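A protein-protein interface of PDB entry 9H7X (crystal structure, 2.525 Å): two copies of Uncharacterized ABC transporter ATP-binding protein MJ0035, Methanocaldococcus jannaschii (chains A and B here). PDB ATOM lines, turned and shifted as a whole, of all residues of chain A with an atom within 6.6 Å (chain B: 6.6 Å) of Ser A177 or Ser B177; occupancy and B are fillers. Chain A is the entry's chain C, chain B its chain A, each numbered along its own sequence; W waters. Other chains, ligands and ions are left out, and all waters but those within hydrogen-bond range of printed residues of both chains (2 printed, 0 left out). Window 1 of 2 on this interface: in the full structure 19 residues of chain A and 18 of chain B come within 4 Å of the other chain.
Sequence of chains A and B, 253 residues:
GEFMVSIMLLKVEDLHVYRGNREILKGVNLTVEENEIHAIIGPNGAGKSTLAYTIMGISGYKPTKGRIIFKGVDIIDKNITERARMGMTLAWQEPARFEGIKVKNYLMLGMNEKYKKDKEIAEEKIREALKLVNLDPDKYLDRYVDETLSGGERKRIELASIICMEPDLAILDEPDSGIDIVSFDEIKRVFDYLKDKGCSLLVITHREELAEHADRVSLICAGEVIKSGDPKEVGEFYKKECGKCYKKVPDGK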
ATOM      1  N   GLN A  93      38.003  28.770 -10.789  1.00  0.00           N
ATOM      2  CA  GLN A  93      36.706  28.206 -10.450  1.00  0.00           C
ATOM      3  C   GLN A  93      36.879  27.066  -9.421  1.00  0.00           C
ATOM      4  O   GLN A  93      36.130  26.997  -8.450  1.00  0.00           O
ATOM      5  CB  GLN A  93      36.001  27.746 -11.728  1.00  0.00           C
ATOM      6  CG  GLN A  93      34.496  27.697 -11.603  1.00  0.00           C
ATOM      7  CD  GLN A  93      34.059  26.423 -10.927  1.00  0.00           C
ATOM      8  OE1 GLN A  93      33.418  26.438  -9.867  1.00  0.00           O
ATOM      9  NE2 GLN A  93      34.446  25.282 -11.501  1.00  0.00           N
ATOM     10  N   GLY A 151      34.420  22.249  -0.641  1.00  0.00           N
ATOM     11  CA  GLY A 151      34.477  23.218  -1.733  1.00  0.00           C
ATOM     12  C   GLY A 151      34.064  24.629  -1.349  1.00  0.00           C
ATOM     13  O   GLY A 151      34.678  25.605  -1.791  1.00  0.00           O
ATOM     14  N   GLY A 152      33.042  24.730  -0.500  1.00  0.00           N
ATOM     15  CA  GLY A 152      32.554  26.016  -0.027  1.00  0.00           C
ATOM     16  C   GLY A 152      33.574  26.698   0.850  1.00  0.00           C
ATOM     17  O   GLY A 152      33.791  27.900   0.722  1.00  0.00           O
ATOM     18  N   LYS A 155      36.445  27.879  -1.340  1.00  0.00           N
ATOM     19  CA  LYS A 155      36.024  29.071  -2.062  1.00  0.00           C
ATOM     20  C   LYS A 155      36.013  30.312  -1.157  1.00  0.00           C
ATOM     21  O   LYS A 155      36.389  31.394  -1.609  1.00  0.00           O
ATOM     22  CB  LYS A 155      34.659  28.846  -2.701  1.00  0.00           C
ATOM     23  CG  LYS A 155      34.595  29.357  -4.129  1.00  0.00           C
ATOM     24  CD  LYS A 155      35.521  28.584  -5.061  1.00  0.00           C
ATOM     25  CE  LYS A 155      35.473  29.182  -6.438  1.00  0.00           C
ATOM     26  NZ  LYS A 155      34.327  28.649  -7.188  1.00  0.00           N
ATOM     27  N   ASP A 173      36.556  33.910 -11.256  1.00  0.00           N
ATOM     28  CA  ASP A 173      35.821  32.977 -12.114  1.00  0.00           C
ATOM     29  C   ASP A 173      34.894  32.138 -11.228  1.00  0.00           C
ATOM     30  O   ASP A 173      35.339  31.203 -10.575  1.00  0.00           O
ATOM     31  CB  ASP A 173      36.815  32.079 -12.878  1.00  0.00           C
ATOM     32  CG  ASP A 173      36.199  31.190 -13.947  1.00  0.00           C
ATOM     33  OD1 ASP A 173      35.018  31.420 -14.305  1.00  0.00           O
ATOM     34  OD2 ASP A 173      36.908  30.270 -14.442  1.00  0.00           O
ATOM     35  N   GLU A 174      33.615  32.495 -11.200  1.00  0.00           N
ATOM     36  CA  GLU A 174      32.578  31.880 -10.378  1.00  0.00           C
ATOM     37  C   GLU A 174      32.949  31.881  -8.914  1.00  0.00           C
ATOM     38  O   GLU A 174      33.165  30.818  -8.337  1.00  0.00           O
ATOM     39  CB  GLU A 174      32.187  30.483 -10.872  1.00  0.00           C
ATOM     40  CG  GLU A 174      31.717  30.469 -12.313  1.00  0.00           C
ATOM     41  CD  GLU A 174      31.082  29.156 -12.711  1.00  0.00           C
ATOM     42  OE1 GLU A 174      30.076  28.764 -12.072  1.00  0.00           O
ATOM     43  OE2 GLU A 174      31.590  28.519 -13.661  1.00  0.00           O
ATOM     44  N   PRO A 175      33.038  33.071  -8.280  1.00  0.00           N
ATOM     45  CA  PRO A 175      33.367  33.102  -6.840  1.00  0.00           C
ATOM     46  C   PRO A 175      32.281  32.472  -5.945  1.00  0.00           C
ATOM     47  O   PRO A 175      32.542  32.119  -4.794  1.00  0.00           O
ATOM     48  CB  PRO A 175      33.531  34.601  -6.562  1.00  0.00           C
ATOM     49  CG  PRO A 175      32.676  35.259  -7.575  1.00  0.00           C
ATOM     50  CD  PRO A 175      32.784  34.429  -8.808  1.00  0.00           C
ATOM     51  N   ASP A 176      31.055  32.347  -6.486  1.00  0.00           N
ATOM     52  CA  ASP A 176      29.863  31.808  -5.831  1.00  0.00           C
ATOM     53  C   ASP A 176      29.784  30.279  -5.859  1.00  0.00           C
ATOM     54  O   ASP A 176      29.088  29.702  -5.037  1.00  0.00           O
ATOM     55  CB  ASP A 176      28.608  32.383  -6.506  1.00  0.00           C
ATOM     56  CG  ASP A 176      28.664  32.385  -8.027  1.00  0.00           C
ATOM     57  OD1 ASP A 176      28.267  31.369  -8.645  1.00  0.00           O
ATOM     58  OD2 ASP A 176      29.104  33.390  -8.593  1.00  0.00           O
ATOM     59  N   SER A 177      30.451  29.642  -6.826  1.00  0.00           N
ATOM     60  CA  SER A 177      30.416  28.210  -7.025  1.00  0.00           C
ATOM     61  C   SER A 177      30.751  27.415  -5.774  1.00  0.00           C
ATOM     62  O   SER A 177      31.813  27.590  -5.187  1.00  0.00           O
ATOM     63  CB  SER A 177      31.345  27.821  -8.164  1.00  0.00           C
ATOM     64  OG  SER A 177      30.911  26.631  -8.806  1.00  0.00           O
ATOM     65  N   GLY A 178      29.827  26.561  -5.352  1.00  0.00           N
ATOM     66  CA  GLY A 178      30.026  25.755  -4.155  1.00  0.00           C
ATOM     67  C   GLY A 178      29.610  26.432  -2.865  1.00  0.00           C
ATOM     68  O   GLY A 178      29.578  25.792  -1.810  1.00  0.00           O
ATOM     69  N   ILE A 179      29.278  27.724  -2.926  1.00  0.00           N
ATOM     70  CA  ILE A 179      28.847  28.465  -1.754  1.00  0.00           C
ATOM     71  C   ILE A 179      27.323  28.429  -1.661  1.00  0.00           C
ATOM     72  O   ILE A 179      26.632  28.553  -2.682  1.00  0.00           O
ATOM     73  CB  ILE A 179      29.472  29.884  -1.729  1.00  0.00           C
ATOM     74  CG1 ILE A 179      30.941  29.784  -1.316  1.00  0.00           C
ATOM     75  CG2 ILE A 179      28.719  30.832  -0.801  1.00  0.00           C
ATOM     76  CD1 ILE A 179      31.713  31.016  -1.549  1.00  0.00           C
ATOM     77  N   PHE A 184      25.148  34.376   0.422  1.00  0.00           N
ATOM     78  CA  PHE A 184      25.350  35.267  -0.705  1.00  0.00           C
ATOM     79  C   PHE A 184      25.485  36.728  -0.309  1.00  0.00           C
ATOM     80  O   PHE A 184      26.119  37.483  -1.052  1.00  0.00           O
ATOM     81  CB  PHE A 184      24.290  35.073  -1.782  1.00  0.00           C
ATOM     82  CG  PHE A 184      24.459  33.853  -2.661  1.00  0.00           C
ATOM     83  CD1 PHE A 184      25.533  32.987  -2.489  1.00  0.00           C
ATOM     84  CD2 PHE A 184      23.545  33.573  -3.658  1.00  0.00           C
ATOM     85  CE1 PHE A 184      25.677  31.863  -3.289  1.00  0.00           C
ATOM     86  CE2 PHE A 184      23.694  32.450  -4.457  1.00  0.00           C
ATOM     87  CZ  PHE A 184      24.762  31.607  -4.272  1.00  0.00           C
ATOM     88  N   ARG A 207      25.053  33.292 -10.996  1.00  0.00           N
ATOM     89  CA  ARG A 207      24.082  33.720 -10.014  1.00  0.00           C
ATOM     90  C   ARG A 207      23.621  35.130 -10.324  1.00  0.00           C
ATOM     91  O   ARG A 207      24.411  36.060 -10.236  1.00  0.00           O
ATOM     92  CB  ARG A 207      24.696  33.687  -8.612  1.00  0.00           C
ATOM     93  CG  ARG A 207      24.929  32.287  -8.071  1.00  0.00           C
ATOM     94  CD  ARG A 207      23.630  31.530  -7.886  1.00  0.00           C
ATOM     95  NE  ARG A 207      23.818  30.317  -7.092  1.00  0.00           N
ATOM     96  CZ  ARG A 207      22.829  29.592  -6.582  1.00  0.00           C
ATOM     97  NH1 ARG A 207      21.567  29.949  -6.778  1.00  0.00           N
ATOM     98  NH2 ARG A 207      23.097  28.509  -5.866  1.00  0.00           N
ATOM     99  N   GLN B  93      31.554  16.535  -7.244  1.00  0.00           N
ATOM    100  CA  GLN B  93      31.512  17.953  -7.541  1.00  0.00           C
ATOM    101  C   GLN B  93      32.990  18.226  -7.879  1.00  0.00           C
ATOM    102  O   GLN B  93      33.872  17.976  -7.044  1.00  0.00           O
ATOM    103  CB  GLN B  93      31.000  18.766  -6.335  1.00  0.00           C
ATOM    104  CG  GLN B  93      31.528  20.202  -6.217  1.00  0.00           C
ATOM    105  CD  GLN B  93      31.152  21.176  -7.320  1.00  0.00           C
ATOM    106  OE1 GLN B  93      31.266  22.402  -7.149  1.00  0.00           O
ATOM    107  NE2 GLN B  93      30.714  20.680  -8.477  1.00  0.00           N
ATOM    108  N   GLU B  94      33.250  18.592  -9.156  1.00  0.00           N
ATOM    109  CA  GLU B  94      34.578  18.780  -9.759  1.00  0.00           C
ATOM    110  C   GLU B  94      35.071  17.394 -10.221  1.00  0.00           C
ATOM    111  O   GLU B  94      35.832  16.722  -9.515  1.00  0.00           O
ATOM    112  CB  GLU B  94      35.569  19.478  -8.796  1.00  0.00           C
ATOM    113  CG  GLU B  94      36.955  19.747  -9.359  1.00  0.00           C
ATOM    114  CD  GLU B  94      38.054  19.694  -8.313  1.00  0.00           C
ATOM    115  OE1 GLU B  94      38.507  20.773  -7.868  1.00  0.00           O
ATOM    116  OE2 GLU B  94      38.456  18.571  -7.929  1.00  0.00           O
ATOM    117  N   GLY B 151      34.277  23.704 -17.486  1.00  0.00           N
ATOM    118  CA  GLY B 151      33.592  23.059 -16.371  1.00  0.00           C
ATOM    119  C   GLY B 151      32.164  22.634 -16.677  1.00  0.00           C
ATOM    120  O   GLY B 151      31.713  21.574 -16.242  1.00  0.00           O
ATOM    121  N   GLY B 152      31.463  23.451 -17.442  1.00  0.00           N
ATOM    122  CA  GLY B 152      30.100  23.154 -17.837  1.00  0.00           C
ATOM    123  C   GLY B 152      30.053  21.963 -18.764  1.00  0.00           C
ATOM    124  O   GLY B 152      29.194  21.098 -18.615  1.00  0.00           O
ATOM    125  N   LYS B 155      30.841  18.815 -16.781  1.00  0.00           N
ATOM    126  CA  LYS B 155      29.668  18.469 -15.982  1.00  0.00           C
ATOM    127  C   LYS B 155      28.577  17.827 -16.852  1.00  0.00           C
ATOM    128  O   LYS B 155      27.918  16.892 -16.406  1.00  0.00           O
ATOM    129  CB  LYS B 155      29.126  19.704 -15.247  1.00  0.00           C
ATOM    130  CG  LYS B 155      28.766  19.435 -13.797  1.00  0.00           C
ATOM    131  CD  LYS B 155      29.981  19.058 -12.979  1.00  0.00           C
ATOM    132  CE  LYS B 155      29.592  18.739 -11.568  1.00  0.00           C
ATOM    133  NZ  LYS B 155      29.457  19.967 -10.761  1.00  0.00           N
ATOM    134  N   ASP B 173      26.586  14.997  -6.732  1.00  0.00           N
ATOM    135  CA  ASP B 173      27.022  16.083  -5.857  1.00  0.00           C
ATOM    136  C   ASP B 173      27.146  17.361  -6.694  1.00  0.00           C
ATOM    137  O   ASP B 173      28.122  17.541  -7.414  1.00  0.00           O
ATOM    138  CB  ASP B 173      28.377  15.723  -5.216  1.00  0.00           C
ATOM    139  CG  ASP B 173      28.850  16.673  -4.133  1.00  0.00           C
ATOM    140  OD1 ASP B 173      28.034  17.512  -3.675  1.00  0.00           O
ATOM    141  OD2 ASP B 173      30.033  16.575  -3.733  1.00  0.00           O
ATOM    142  N   GLU B 174      26.141  18.227  -6.603  1.00  0.00           N
ATOM    143  CA  GLU B 174      26.023  19.466  -7.362  1.00  0.00           C
ATOM    144  C   GLU B 174      26.120  19.223  -8.849  1.00  0.00           C
ATOM    145  O   GLU B 174      27.074  19.658  -9.472  1.00  0.00           O
ATOM    146  CB  GLU B 174      27.000  20.547  -6.885  1.00  0.00           C
ATOM    147  CG  GLU B 174      26.873  20.870  -5.412  1.00  0.00           C
ATOM    148  CD  GLU B 174      27.642  22.108  -5.005  1.00  0.00           C
ATOM    149  OE1 GLU B 174      27.358  23.189  -5.574  1.00  0.00           O
ATOM    150  OE2 GLU B 174      28.534  22.002  -4.130  1.00  0.00           O
ATOM    151  N   PRO B 175      25.137  18.522  -9.450  1.00  0.00           N
ATOM    152  CA  PRO B 175      25.189  18.298 -10.905  1.00  0.00           C
ATOM    153  C   PRO B 175      25.043  19.580 -11.730  1.00  0.00           C
ATOM    154  O   PRO B 175      25.395  19.594 -12.911  1.00  0.00           O
ATOM    155  CB  PRO B 175      24.016  17.351 -11.145  1.00  0.00           C
ATOM    156  CG  PRO B 175      23.061  17.658 -10.037  1.00  0.00           C
ATOM    157  CD  PRO B 175      23.904  17.961  -8.856  1.00  0.00           C
ATOM    158  N   ASP B 176      24.516  20.653 -11.098  1.00  0.00           N
ATOM    159  CA  ASP B 176      24.260  21.973 -11.670  1.00  0.00           C
ATOM    160  C   ASP B 176      25.475  22.885 -11.683  1.00  0.00           C
ATOM    161  O   ASP B 176      25.511  23.830 -12.470  1.00  0.00           O
ATOM    162  CB  ASP B 176      23.137  22.665 -10.889  1.00  0.00           C
ATOM    163  CG  ASP B 176      23.277  22.547  -9.381  1.00  0.00           C
ATOM    164  OD1 ASP B 176      23.943  23.415  -8.774  1.00  0.00           O
ATOM    165  OD2 ASP B 176      22.728  21.597  -8.814  1.00  0.00           O
ATOM    166  N   SER B 177      26.441  22.643 -10.789  1.00  0.00           N
ATOM    167  CA  SER B 177      27.634  23.459 -10.642  1.00  0.00           C
ATOM    168  C   SER B 177      28.386  23.672 -11.952  1.00  0.00           C
ATOM    169  O   SER B 177      28.778  22.709 -12.609  1.00  0.00           O
ATOM    170  CB  SER B 177      28.553  22.852  -9.597  1.00  0.00           C
ATOM    171  OG  SER B 177      29.314  23.864  -8.957  1.00  0.00           O
ATOM    172  N   GLY B 178      28.543  24.937 -12.331  1.00  0.00           N
ATOM    173  CA  GLY B 178      29.222  25.306 -13.565  1.00  0.00           C
ATOM    174  C   GLY B 178      28.340  25.315 -14.794  1.00  0.00           C
ATOM    175  O   GLY B 178      28.783  25.729 -15.866  1.00  0.00           O
ATOM    176  N   ILE B 179      27.095  24.849 -14.664  1.00  0.00           N
ATOM    177  CA  ILE B 179      26.167  24.832 -15.779  1.00  0.00           C
ATOM    178  C   ILE B 179      25.339  26.122 -15.778  1.00  0.00           C
ATOM    179  O   ILE B 179      24.936  26.605 -14.718  1.00  0.00           O
ATOM    180  CB  ILE B 179      25.345  23.523 -15.794  1.00  0.00           C
ATOM    181  CG1 ILE B 179      26.224  22.360 -16.307  1.00  0.00           C
ATOM    182  CG2 ILE B 179      24.067  23.651 -16.628  1.00  0.00           C
ATOM    183  CD1 ILE B 179      25.648  21.024 -16.108  1.00  0.00           C
ATOM    184  N   PHE B 184      19.049  24.764 -17.502  1.00  0.00           N
ATOM    185  CA  PHE B 184      18.533  24.035 -16.347  1.00  0.00           C
ATOM    186  C   PHE B 184      17.379  23.104 -16.691  1.00  0.00           C
ATOM    187  O   PHE B 184      17.162  22.132 -15.973  1.00  0.00           O
ATOM    188  CB  PHE B 184      18.175  24.991 -15.205  1.00  0.00           C
ATOM    189  CG  PHE B 184      19.348  25.480 -14.378  1.00  0.00           C
ATOM    190  CD1 PHE B 184      20.642  25.055 -14.646  1.00  0.00           C
ATOM    191  CD2 PHE B 184      19.154  26.350 -13.323  1.00  0.00           C
ATOM    192  CE1 PHE B 184      21.712  25.520 -13.898  1.00  0.00           C
ATOM    193  CE2 PHE B 184      20.231  26.810 -12.576  1.00  0.00           C
ATOM    194  CZ  PHE B 184      21.498  26.387 -12.863  1.00  0.00           C
ATOM    195  N   ARG B 207      20.758  24.905  -6.114  1.00  0.00           N
ATOM    196  CA  ARG B 207      19.807  25.525  -7.009  1.00  0.00           C
ATOM    197  C   ARG B 207      18.395  25.108  -6.623  1.00  0.00           C
ATOM    198  O   ARG B 207      18.047  23.933  -6.738  1.00  0.00           O
ATOM    199  CB  ARG B 207      20.074  25.094  -8.453  1.00  0.00           C
ATOM    200  CG  ARG B 207      21.320  25.705  -9.056  1.00  0.00           C
ATOM    201  CD  ARG B 207      21.214  27.210  -9.175  1.00  0.00           C
ATOM    202  NE  ARG B 207      22.273  27.756 -10.023  1.00  0.00           N
ATOM    203  CZ  ARG B 207      22.309  29.004 -10.478  1.00  0.00           C
ATOM    204  NH1 ARG B 207      21.342  29.860 -10.168  1.00  0.00           N
ATOM    205  NH2 ARG B 207      23.313  29.408 -11.246  1.00  0.00           N
HETATM  206  O   HOH W   1      33.391  24.762  -6.310  1.00  0.00           O
HETATM  207  O   HOH W   2      27.199  25.600  -6.353  1.00  0.00           O
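OG of Ser B177 is in hydrogen-bond range of OG of Ser A177.
The guanidinium group (NH1) of Arg A207 lies close to the guanidinium group (NH1) of Arg B207 (3.4 Å).
NZ of Lys A155 sits close to O of Ser A177 (3.4 Å).
The side-chain amino group (NZ) of Lys B155 is in hydrogen-bond range of the backbone carbonyl oxygen (O) of Glu B174 (2.7 Å).
The side-chain amide oxygen (OE1) of Gln B93 sits at hydrogen-bond distance from the side-chain hydroxyl (OG) of Ser B177, at 3.0 Å.
O of Ser B177 lies close to NZ of Lys B155, at 3.4 Å.
The side-chain amino group (NZ) of Lys A155 is in hydrogen-bond range of the backbone carbonyl oxygen (O) of Glu A174.
The side-chain amide oxygen of Gln A93 is in hydrogen-bond range of the side-chain hydroxyl of Ser A177.
Among the printed residues, pairs that only touch across the chains: Glu A174 with Gly B178 (3.9 Å) and Gly A178 with Glu B174 (3.96 Å).
Pro A175 touches none of the printed residues of chain B.
Printed residues of chain B within 4 Å of Ser A177: Ser B177 (3.2 Å).
Printed residues of chain B within 4 Å of Gly A178: Glu B174 (3.96 Å).
Ile A179 touches none of the printed residues of chain B.
Of the printed residues of chain B, Arg A207 touches Arg B207.
Of the printed residues of chain A, Glu B174 touches Gly A178.
Of chain A, only Ser A177 comes within 4 Å of Ser B177.
Of the printed residues of chain A, Gly B178 touches Glu A174.
The nearest residue of chain A that does not touch Ser B177 is Gly A178 (4.5 Å).
Of the 14 printed residues of chain B, 4 touch a printed residue of chain A.
Among the printed residues, 4 pairs touch across the chains.
Among the printed residues, no Asp or Glu carboxylate lies within 4 Å of a Lys or Arg side-chain nitrogen of the other chain.
Glu A174 touches Gly B178, and with the chains exchanged Gly A178 touches Glu B174.
Ser A177 touches its own counterpart, Ser B177.
Arg A207 touches its own counterpart, Arg B207.
Of the 4 pairs that touch across the chains among the printed residues, 4 have their exchanged pair printed and touching as well.
Water W2 lies within hydrogen-bond range of OE1 of Glu B174 (2.5 Å) and N of Gly A178 (3.0 Å).
Water W1 lies within hydrogen-bond range of the side-chain amide oxygen (OE1) of Gln B93 (3.3 Å) and the backbone carbonyl oxygen (O) of Ser A177 (3.4 Å).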
